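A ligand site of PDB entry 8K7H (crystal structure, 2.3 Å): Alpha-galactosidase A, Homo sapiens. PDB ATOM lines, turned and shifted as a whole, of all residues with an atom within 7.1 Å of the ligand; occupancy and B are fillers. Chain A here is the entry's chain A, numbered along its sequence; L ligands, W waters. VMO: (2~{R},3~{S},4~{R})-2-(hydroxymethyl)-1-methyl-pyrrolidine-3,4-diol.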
ATOM      1  N   LEU A  14      -3.449   9.683   4.808  1.00  0.00           N
ATOM      2  CA  LEU A  14      -3.075   9.352   3.446  1.00  0.00           C
ATOM      3  C   LEU A  14      -2.690   7.877   3.413  1.00  0.00           C
ATOM      4  O   LEU A  14      -1.915   7.424   4.269  1.00  0.00           O
ATOM      5  CB  LEU A  14      -1.911  10.232   2.970  1.00  0.00           C
ATOM      6  CG  LEU A  14      -1.387  10.097   1.551  1.00  0.00           C
ATOM      7  CD1 LEU A  14      -2.474  10.397   0.526  1.00  0.00           C
ATOM      8  CD2 LEU A  14      -0.204  11.040   1.364  1.00  0.00           C
ATOM      9  N   TRP A  16      -0.901   5.888   1.426  1.00  0.00           N
ATOM     10  CA  TRP A  16       0.160   5.300   0.625  1.00  0.00           C
ATOM     11  C   TRP A  16       1.100   4.419   1.439  1.00  0.00           C
ATOM     12  O   TRP A  16       1.270   3.232   1.128  1.00  0.00           O
ATOM     13  CB  TRP A  16       0.966   6.367  -0.107  1.00  0.00           C
ATOM     14  CG  TRP A  16       1.977   5.696  -0.983  1.00  0.00           C
ATOM     15  CD1 TRP A  16       3.325   5.657  -0.804  1.00  0.00           C
ATOM     16  CD2 TRP A  16       1.695   4.881  -2.125  1.00  0.00           C
ATOM     17  NE1 TRP A  16       3.906   4.909  -1.798  1.00  0.00           N
ATOM     18  CE2 TRP A  16       2.929   4.413  -2.622  1.00  0.00           C
ATOM     19  CE3 TRP A  16       0.527   4.515  -2.802  1.00  0.00           C
ATOM     20  CZ2 TRP A  16       3.031   3.606  -3.751  1.00  0.00           C
ATOM     21  CZ3 TRP A  16       0.621   3.709  -3.926  1.00  0.00           C
ATOM     22  CH2 TRP A  16       1.871   3.267  -4.388  1.00  0.00           C
ATOM     23  N   GLU A  17       1.745   4.980   2.464  1.00  0.00           N
ATOM     24  CA  GLU A  17       2.815   4.241   3.132  1.00  0.00           C
ATOM     25  C   GLU A  17       2.319   2.924   3.709  1.00  0.00           C
ATOM     26  O   GLU A  17       2.990   1.898   3.601  1.00  0.00           O
ATOM     27  CB  GLU A  17       3.474   5.096   4.224  1.00  0.00           C
ATOM     28  CG  GLU A  17       4.837   4.574   4.687  1.00  0.00           C
ATOM     29  CD  GLU A  17       4.747   3.327   5.553  1.00  0.00           C
ATOM     30  OE1 GLU A  17       3.816   3.244   6.379  1.00  0.00           O
ATOM     31  OE2 GLU A  17       5.604   2.421   5.411  1.00  0.00           O
ATOM     32  N   CYS A  21      -0.155   0.107  -3.101  1.00  0.00           N
ATOM     33  CA  CYS A  21      -0.959  -0.159  -4.295  1.00  0.00           C
ATOM     34  C   CYS A  21      -1.568  -1.549  -4.252  1.00  0.00           C
ATOM     35  O   CYS A  21      -1.478  -2.301  -5.218  1.00  0.00           O
ATOM     36  CB  CYS A  21      -0.099   0.000  -5.549  1.00  0.00           C
ATOM     37  SG  CYS A  21      -1.028   0.156  -7.084  1.00  0.00           S
ATOM     38  N   ASP A  61      -4.395   8.211  -2.262  1.00  0.00           N
ATOM     39  CA  ASP A  61      -3.154   8.282  -3.005  1.00  0.00           C
ATOM     40  C   ASP A  61      -3.292   7.515  -4.313  1.00  0.00           C
ATOM     41  O   ASP A  61      -4.390   7.365  -4.839  1.00  0.00           O
ATOM     42  CB  ASP A  61      -1.980   7.752  -2.171  1.00  0.00           C
ATOM     43  CG  ASP A  61      -0.663   8.411  -2.513  1.00  0.00           C
ATOM     44  OD1 ASP A  61      -0.076   8.060  -3.565  1.00  0.00           O
ATOM     45  OD2 ASP A  61      -0.213   9.302  -1.761  1.00  0.00           O
ATOM     46  N   ASP A  62      -2.174   7.019  -4.845  1.00  0.00           N
ATOM     47  CA  ASP A  62      -2.174   6.357  -6.148  1.00  0.00           C
ATOM     48  C   ASP A  62      -2.966   5.046  -6.094  1.00  0.00           C
ATOM     49  O   ASP A  62      -3.241   4.484  -5.025  1.00  0.00           O
ATOM     50  CB  ASP A  62      -0.739   6.081  -6.601  1.00  0.00           C
ATOM     51  CG  ASP A  62      -0.616   5.877  -8.098  1.00  0.00           C
ATOM     52  OD1 ASP A  62      -1.664   5.794  -8.785  1.00  0.00           O
ATOM     53  OD2 ASP A  62       0.523   5.812  -8.590  1.00  0.00           O
ATOM     54  N   CYS A  63      -3.370   4.576  -7.277  1.00  0.00           N
ATOM     55  CA  CYS A  63      -4.053   3.306  -7.501  1.00  0.00           C
ATOM     56  C   CYS A  63      -5.527   3.339  -7.106  1.00  0.00           C
ATOM     57  O   CYS A  63      -6.054   2.355  -6.597  1.00  0.00           O
ATOM     58  CB  CYS A  63      -3.337   2.152  -6.788  1.00  0.00           C
ATOM     59  SG  CYS A  63      -1.556   2.121  -7.138  1.00  0.00           S
ATOM     60  N   TYR A 103      -5.467  11.986  -5.789  1.00  0.00           N
ATOM     61  CA  TYR A 103      -4.125  11.906  -6.342  1.00  0.00           C
ATOM     62  C   TYR A 103      -4.186  11.937  -7.866  1.00  0.00           C
ATOM     63  O   TYR A 103      -5.098  11.383  -8.477  1.00  0.00           O
ATOM     64  CB  TYR A 103      -3.417  10.629  -5.843  1.00  0.00           C
ATOM     65  CG  TYR A 103      -2.136  10.233  -6.539  1.00  0.00           C
ATOM     66  CD1 TYR A 103      -2.141   9.572  -7.764  1.00  0.00           C
ATOM     67  CD2 TYR A 103      -0.902  10.477  -5.942  1.00  0.00           C
ATOM     68  CE1 TYR A 103      -0.970   9.204  -8.394  1.00  0.00           C
ATOM     69  CE2 TYR A 103       0.281  10.112  -6.556  1.00  0.00           C
ATOM     70  CZ  TYR A 103       0.240   9.470  -7.782  1.00  0.00           C
ATOM     71  OH  TYR A 103       1.416   9.104  -8.404  1.00  0.00           O
ATOM     72  N   ASP A 105      -1.167  12.798 -11.488  1.00  0.00           N
ATOM     73  CA  ASP A 105       0.230  12.875 -11.882  1.00  0.00           C
ATOM     74  C   ASP A 105       0.410  13.844 -13.048  1.00  0.00           C
ATOM     75  O   ASP A 105      -0.359  13.817 -14.004  1.00  0.00           O
ATOM     76  CB  ASP A 105       0.783  11.492 -12.259  1.00  0.00           C
ATOM     77  CG  ASP A 105       2.298  11.466 -12.345  1.00  0.00           C
ATOM     78  OD1 ASP A 105       2.845  12.072 -13.286  1.00  0.00           O
ATOM     79  OD2 ASP A 105       2.927  10.830 -11.477  1.00  0.00           O
ATOM     80  N   THR A 110       0.680   7.868 -13.867  1.00  0.00           N
ATOM     81  CA  THR A 110       1.011   7.886 -12.453  1.00  0.00           C
ATOM     82  C   THR A 110       2.206   6.964 -12.202  1.00  0.00           C
ATOM     83  O   THR A 110       2.554   6.125 -13.044  1.00  0.00           O
ATOM     84  CB  THR A 110      -0.169   7.470 -11.586  1.00  0.00           C
ATOM     85  OG1 THR A 110      -0.345   6.050 -11.661  1.00  0.00           O
ATOM     86  CG2 THR A 110      -1.453   8.156 -12.047  1.00  0.00           C
ATOM     87  N   CYS A 111       2.840   7.141 -11.042  1.00  0.00           N
ATOM     88  CA  CYS A 111       4.004   6.332 -10.711  1.00  0.00           C
ATOM     89  C   CYS A 111       3.695   4.836 -10.737  1.00  0.00           C
ATOM     90  O   CYS A 111       4.573   4.025 -11.048  1.00  0.00           O
ATOM     91  CB  CYS A 111       4.579   6.730  -9.354  1.00  0.00           C
ATOM     92  SG  CYS A 111       5.240   8.430  -9.298  1.00  0.00           S
ATOM     93  N   ALA A 112       2.463   4.448 -10.416  1.00  0.00           N
ATOM     94  CA  ALA A 112       2.055   3.056 -10.472  1.00  0.00           C
ATOM     95  C   ALA A 112       1.577   2.607 -11.843  1.00  0.00           C
ATOM     96  O   ALA A 112       1.301   1.420 -12.033  1.00  0.00           O
ATOM     97  CB  ALA A 112       0.973   2.769  -9.435  1.00  0.00           C
ATOM     98  N   GLY A 113       1.442   3.521 -12.802  1.00  0.00           N
ATOM     99  CA  GLY A 113       1.125   3.157 -14.168  1.00  0.00           C
ATOM    100  C   GLY A 113      -0.293   3.437 -14.625  1.00  0.00           C
ATOM    101  O   GLY A 113      -0.678   2.964 -15.696  1.00  0.00           O
ATOM    102  N   LYS A 137      -3.050  15.792  -4.461  1.00  0.00           N
ATOM    103  CA  LYS A 137      -1.630  15.484  -4.455  1.00  0.00           C
ATOM    104  C   LYS A 137      -1.218  15.193  -5.890  1.00  0.00           C
ATOM    105  O   LYS A 137      -1.798  14.297  -6.530  1.00  0.00           O
ATOM    106  CB  LYS A 137      -1.328  14.293  -3.539  1.00  0.00           C
ATOM    107  CG  LYS A 137       0.156  13.943  -3.423  1.00  0.00           C
ATOM    108  CD  LYS A 137       0.342  12.565  -2.793  1.00  0.00           C
ATOM    109  CE  LYS A 137       1.801  12.259  -2.514  1.00  0.00           C
ATOM    110  NZ  LYS A 137       1.983  10.932  -1.877  1.00  0.00           N
ATOM    111  N   ASP A 139       1.643  14.111  -8.429  1.00  0.00           N
ATOM    112  CA  ASP A 139       2.906  13.412  -8.518  1.00  0.00           C
ATOM    113  C   ASP A 139       3.643  13.775  -9.813  1.00  0.00           C
ATOM    114  O   ASP A 139       3.069  14.341 -10.750  1.00  0.00           O
ATOM    115  CB  ASP A 139       2.667  11.904  -8.431  1.00  0.00           C
ATOM    116  CG  ASP A 139       3.777  11.176  -7.693  1.00  0.00           C
ATOM    117  OD1 ASP A 139       4.866  11.757  -7.523  1.00  0.00           O
ATOM    118  OD2 ASP A 139       3.543  10.019  -7.289  1.00  0.00           O
ATOM    119  N   GLY A 140       4.930  13.427  -9.865  1.00  0.00           N
ATOM    120  CA  GLY A 140       5.779  13.842 -10.963  1.00  0.00           C
ATOM    121  C   GLY A 140       6.391  12.759 -11.837  1.00  0.00           C
ATOM    122  O   GLY A 140       7.357  13.032 -12.557  1.00  0.00           O
ATOM    123  N   CYS A 141       5.850  11.540 -11.809  1.00  0.00           N
ATOM    124  CA  CYS A 141       6.437  10.477 -12.618  1.00  0.00           C
ATOM    125  C   CYS A 141       6.106  10.653 -14.089  1.00  0.00           C
ATOM    126  O   CYS A 141       5.160  11.358 -14.466  1.00  0.00           O
ATOM    127  CB  CYS A 141       5.939   9.102 -12.156  1.00  0.00           C
ATOM    128  SG  CYS A 141       6.731   8.450 -10.675  1.00  0.00           S
ATOM    129  N   GLU A 172       4.800  17.643  -5.858  1.00  0.00           N
ATOM    130  CA  GLU A 172       6.080  16.958  -5.723  1.00  0.00           C
ATOM    131  C   GLU A 172       7.149  17.570  -6.615  1.00  0.00           C
ATOM    132  O   GLU A 172       8.225  16.989  -6.771  1.00  0.00           O
ATOM    133  CB  GLU A 172       5.916  15.465  -6.009  1.00  0.00           C
ATOM    134  CG  GLU A 172       4.991  14.745  -5.043  1.00  0.00           C
ATOM    135  CD  GLU A 172       5.367  13.288  -4.821  1.00  0.00           C
ATOM    136  OE1 GLU A 172       6.577  12.982  -4.847  1.00  0.00           O
ATOM    137  OE2 GLU A 172       4.463  12.462  -4.624  1.00  0.00           O
ATOM    138  N   LEU A 175      10.972  17.873  -5.537  1.00  0.00           N
ATOM    139  CA  LEU A 175      11.600  16.560  -5.464  1.00  0.00           C
ATOM    140  C   LEU A 175      12.010  16.075  -6.841  1.00  0.00           C
ATOM    141  O   LEU A 175      13.115  15.543  -7.015  1.00  0.00           O
ATOM    142  CB  LEU A 175      10.644  15.560  -4.808  1.00  0.00           C
ATOM    143  CG  LEU A 175      11.075  14.102  -4.866  1.00  0.00           C
ATOM    144  CD1 LEU A 175      12.411  13.919  -4.162  1.00  0.00           C
ATOM    145  CD2 LEU A 175      10.016  13.193  -4.261  1.00  0.00           C
ATOM    146  N   TYR A 176      11.140  16.242  -7.842  1.00  0.00           N
ATOM    147  CA  TYR A 176      11.466  15.761  -9.181  1.00  0.00           C
ATOM    148  C   TYR A 176      12.359  16.725  -9.935  1.00  0.00           C
ATOM    149  O   TYR A 176      12.884  16.361 -11.002  1.00  0.00           O
ATOM    150  CB  TYR A 176      10.189  15.488  -9.968  1.00  0.00           C
ATOM    151  CG  TYR A 176       9.446  14.253  -9.484  1.00  0.00           C
ATOM    152  CD1 TYR A 176       8.504  14.339  -8.474  1.00  0.00           C
ATOM    153  CD2 TYR A 176       9.717  13.003 -10.023  1.00  0.00           C
ATOM    154  CE1 TYR A 176       7.833  13.221  -8.026  1.00  0.00           C
ATOM    155  CE2 TYR A 176       9.054  11.875  -9.579  1.00  0.00           C
ATOM    156  CZ  TYR A 176       8.111  11.990  -8.574  1.00  0.00           C
ATOM    157  OH  TYR A 176       7.454  10.863  -8.122  1.00  0.00           O
ATOM    158  N   ARG A 196       6.699  18.383  -1.730  1.00  0.00           N
ATOM    159  CA  ARG A 196       7.631  17.350  -1.313  1.00  0.00           C
ATOM    160  C   ARG A 196       9.047  17.684  -1.750  1.00  0.00           C
ATOM    161  O   ARG A 196       9.296  17.986  -2.922  1.00  0.00           O
ATOM    162  CB  ARG A 196       7.204  16.001  -1.892  1.00  0.00           C
ATOM    163  CG  ARG A 196       5.975  15.400  -1.235  1.00  0.00           C
ATOM    164  CD  ARG A 196       6.367  14.637   0.021  1.00  0.00           C
ATOM    165  NE  ARG A 196       7.471  13.727  -0.241  1.00  0.00           N
ATOM    166  CZ  ARG A 196       7.348  12.560  -0.852  1.00  0.00           C
ATOM    167  NH1 ARG A 196       6.159  12.080  -1.205  1.00  0.00           N
ATOM    168  NH2 ARG A 196       8.444  11.841  -1.116  1.00  0.00           N
ATOM    169  N   ASP A 200      10.642   9.388  -0.811  1.00  0.00           N
ATOM    170  CA  ASP A 200       9.508   8.831  -0.081  1.00  0.00           C
ATOM    171  C   ASP A 200       9.943   8.275   1.273  1.00  0.00           C
ATOM    172  O   ASP A 200      10.973   7.615   1.403  1.00  0.00           O
ATOM    173  CB  ASP A 200       8.863   7.704  -0.899  1.00  0.00           C
ATOM    174  CG  ASP A 200       8.244   8.195  -2.193  1.00  0.00           C
ATOM    175  OD1 ASP A 200       8.206   9.424  -2.418  1.00  0.00           O
ATOM    176  OD2 ASP A 200       7.783   7.339  -2.980  1.00  0.00           O
ATOM    177  N   ILE A 201       9.127   8.547   2.296  1.00  0.00           N
ATOM    178  CA  ILE A 201       9.357   7.949   3.597  1.00  0.00           C
ATOM    179  C   ILE A 201       8.966   6.477   3.541  1.00  0.00           C
ATOM    180  O   ILE A 201       8.091   6.072   2.776  1.00  0.00           O
ATOM    181  CB  ILE A 201       8.570   8.706   4.682  1.00  0.00           C
ATOM    182  CG1 ILE A 201       9.036   8.299   6.077  1.00  0.00           C
ATOM    183  CG2 ILE A 201       7.071   8.445   4.539  1.00  0.00           C
ATOM    184  CD1 ILE A 201       8.649   9.284   7.152  1.00  0.00           C
ATOM    185  N   ASP A 235       6.984  14.461   4.129  1.00  0.00           N
ATOM    186  CA  ASP A 235       6.228  13.240   3.902  1.00  0.00           C
ATOM    187  C   ASP A 235       5.504  12.738   5.147  1.00  0.00           C
ATOM    188  O   ASP A 235       5.527  13.393   6.195  1.00  0.00           O
ATOM    189  CB  ASP A 235       7.120  12.127   3.327  1.00  0.00           C
ATOM    190  CG  ASP A 235       6.381  11.237   2.351  1.00  0.00           C
ATOM    191  OD1 ASP A 235       5.152  11.415   2.198  1.00  0.00           O
ATOM    192  OD2 ASP A 235       7.027  10.356   1.733  1.00  0.00           O
ATOM    193  N   MET A 236       4.866  11.577   5.036  1.00  0.00           N
ATOM    194  CA  MET A 236       3.827  11.162   5.961  1.00  0.00           C
ATOM    195  C   MET A 236       4.371  10.824   7.336  1.00  0.00           C
ATOM    196  O   MET A 236       5.522  10.424   7.496  1.00  0.00           O
ATOM    197  CB  MET A 236       3.068   9.952   5.406  1.00  0.00           C
ATOM    198  CG  MET A 236       2.363  10.213   4.076  1.00  0.00           C
ATOM    199  SD  MET A 236       2.017   8.694   3.173  1.00  0.00           S
ATOM    200  CE  MET A 236       3.562   8.447   2.293  1.00  0.00           C
HETATM  201  CAA VMO L   1       3.730   7.186  -4.779  1.00  0.00           C
HETATM  202  CAB VMO L   1       3.363   7.955  -3.532  1.00  0.00           C
HETATM  203  CAD VMO L   1       4.685   8.575  -3.202  1.00  0.00           C
HETATM  204  CAE VMO L   1       5.050   9.135  -4.554  1.00  0.00           C
HETATM  205  CAF VMO L   1       2.465   6.927  -5.603  1.00  0.00           C
HETATM  206  CAG VMO L   1       5.863   7.311  -5.873  1.00  0.00           C
HETATM  207  NAH VMO L   1       4.664   8.074  -5.501  1.00  0.00           N
HETATM  208  OAJ VMO L   1       2.421   8.978  -3.877  1.00  0.00           O
HETATM  209  OAK VMO L   1       4.521   9.636  -2.257  1.00  0.00           O
HETATM  210  OAL VMO L   1       2.800   6.188  -6.780  1.00  0.00           O
HETATM  211  O   HOH W   1       7.815  10.717  -4.924  1.00  0.00           O
HETATM  212  O   HOH W   2       4.206   4.033  -7.014  1.00  0.00           O
HETATM  213  O   HOH W   3       5.807   8.857  -0.004  1.00  0.00           O
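The side-chain carboxylate (OD1) of Asp 61 sits at hydrogen-bond distance from an oxygen (OAJ) of the ligand (2.7 Å). NZ of Lys 137 is in hydrogen-bond range of OAJ of the ligand, at 2.8 Å. The side-chain carboxylate of Asp 139 is in salt-bridge range of a nitrogen (NAH) of the ligand (2.9 Å). OAL of the ligand sits at hydrogen-bond distance from OD2 of Asp 62, 2.9 Å away. An oxygen (OAK) of the ligand is in hydrogen-bond range of the guanidinium group of Arg 196, 3.1 Å away.
The side-chain carboxylate (OD2) of Asp 61 is in salt-bridge range of the side-chain amino group (NZ) of Lys 137 (2.7 Å). The side-chain carboxylate of Asp 139 sits at hydrogen-bond distance from the side-chain hydroxyl of Tyr 103 (2.6 Å). The side-chain carboxylate of Asp 139 is in hydrogen-bond range of the side-chain hydroxyl of Tyr 176 (2.8 Å). The side-chain carboxylate of Asp 62 sits at hydrogen-bond distance from the side-chain hydroxyl of Tyr 103, at 3.4 Å. The side-chain carboxylate of Asp 62 is in hydrogen-bond range of the backbone NH of Ala 112 (3.0 Å). OD1 of Asp 62 is in hydrogen-bond range of OG1 of Thr 110. The guanidinium group (NH2) of Arg 196 is in salt-bridge range of the side-chain carboxylate (OD1) of Asp 200 (2.8 Å). OD2 of Asp 235 lies within salt-bridge range of NH2 of Arg 196, at 3.5 Å.
Residues that only touch the ligand: Cys 111 (3.2 Å), Asp 200 (3.3 Å), Glu 172 (3.4 Å), Trp 16 (3.5 Å) and Tyr 103 (3.6 Å). Hydrophobic or aromatic side chains within 4 Å of the ligand: Trp 16 and Tyr 103. Of the 25 residues printed, 10 come within 4 Å of the ligand. Along chain A the residues within 4 Å of the ligand span positions 16 to 200. The nearest printed residue that does not touch the ligand is Ala 112 (4.04 Å).
Water W3 lies within hydrogen-bond range of the side-chain carboxylate (OD2) of Asp 235 (2.6 Å), an oxygen (OAK) of the ligand (2.7 Å), the side-chain carboxylate (OD1) of Asp 200 (3.5 Å) and the guanidinium group (NH1) of Arg 196 (3.5 Å). Water W1 lies within hydrogen-bond range of OE1 of Glu 172 (2.6 Å), OD1 of Asp 200 (2.8 Å) and OH of Tyr 176 (3.2 Å).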
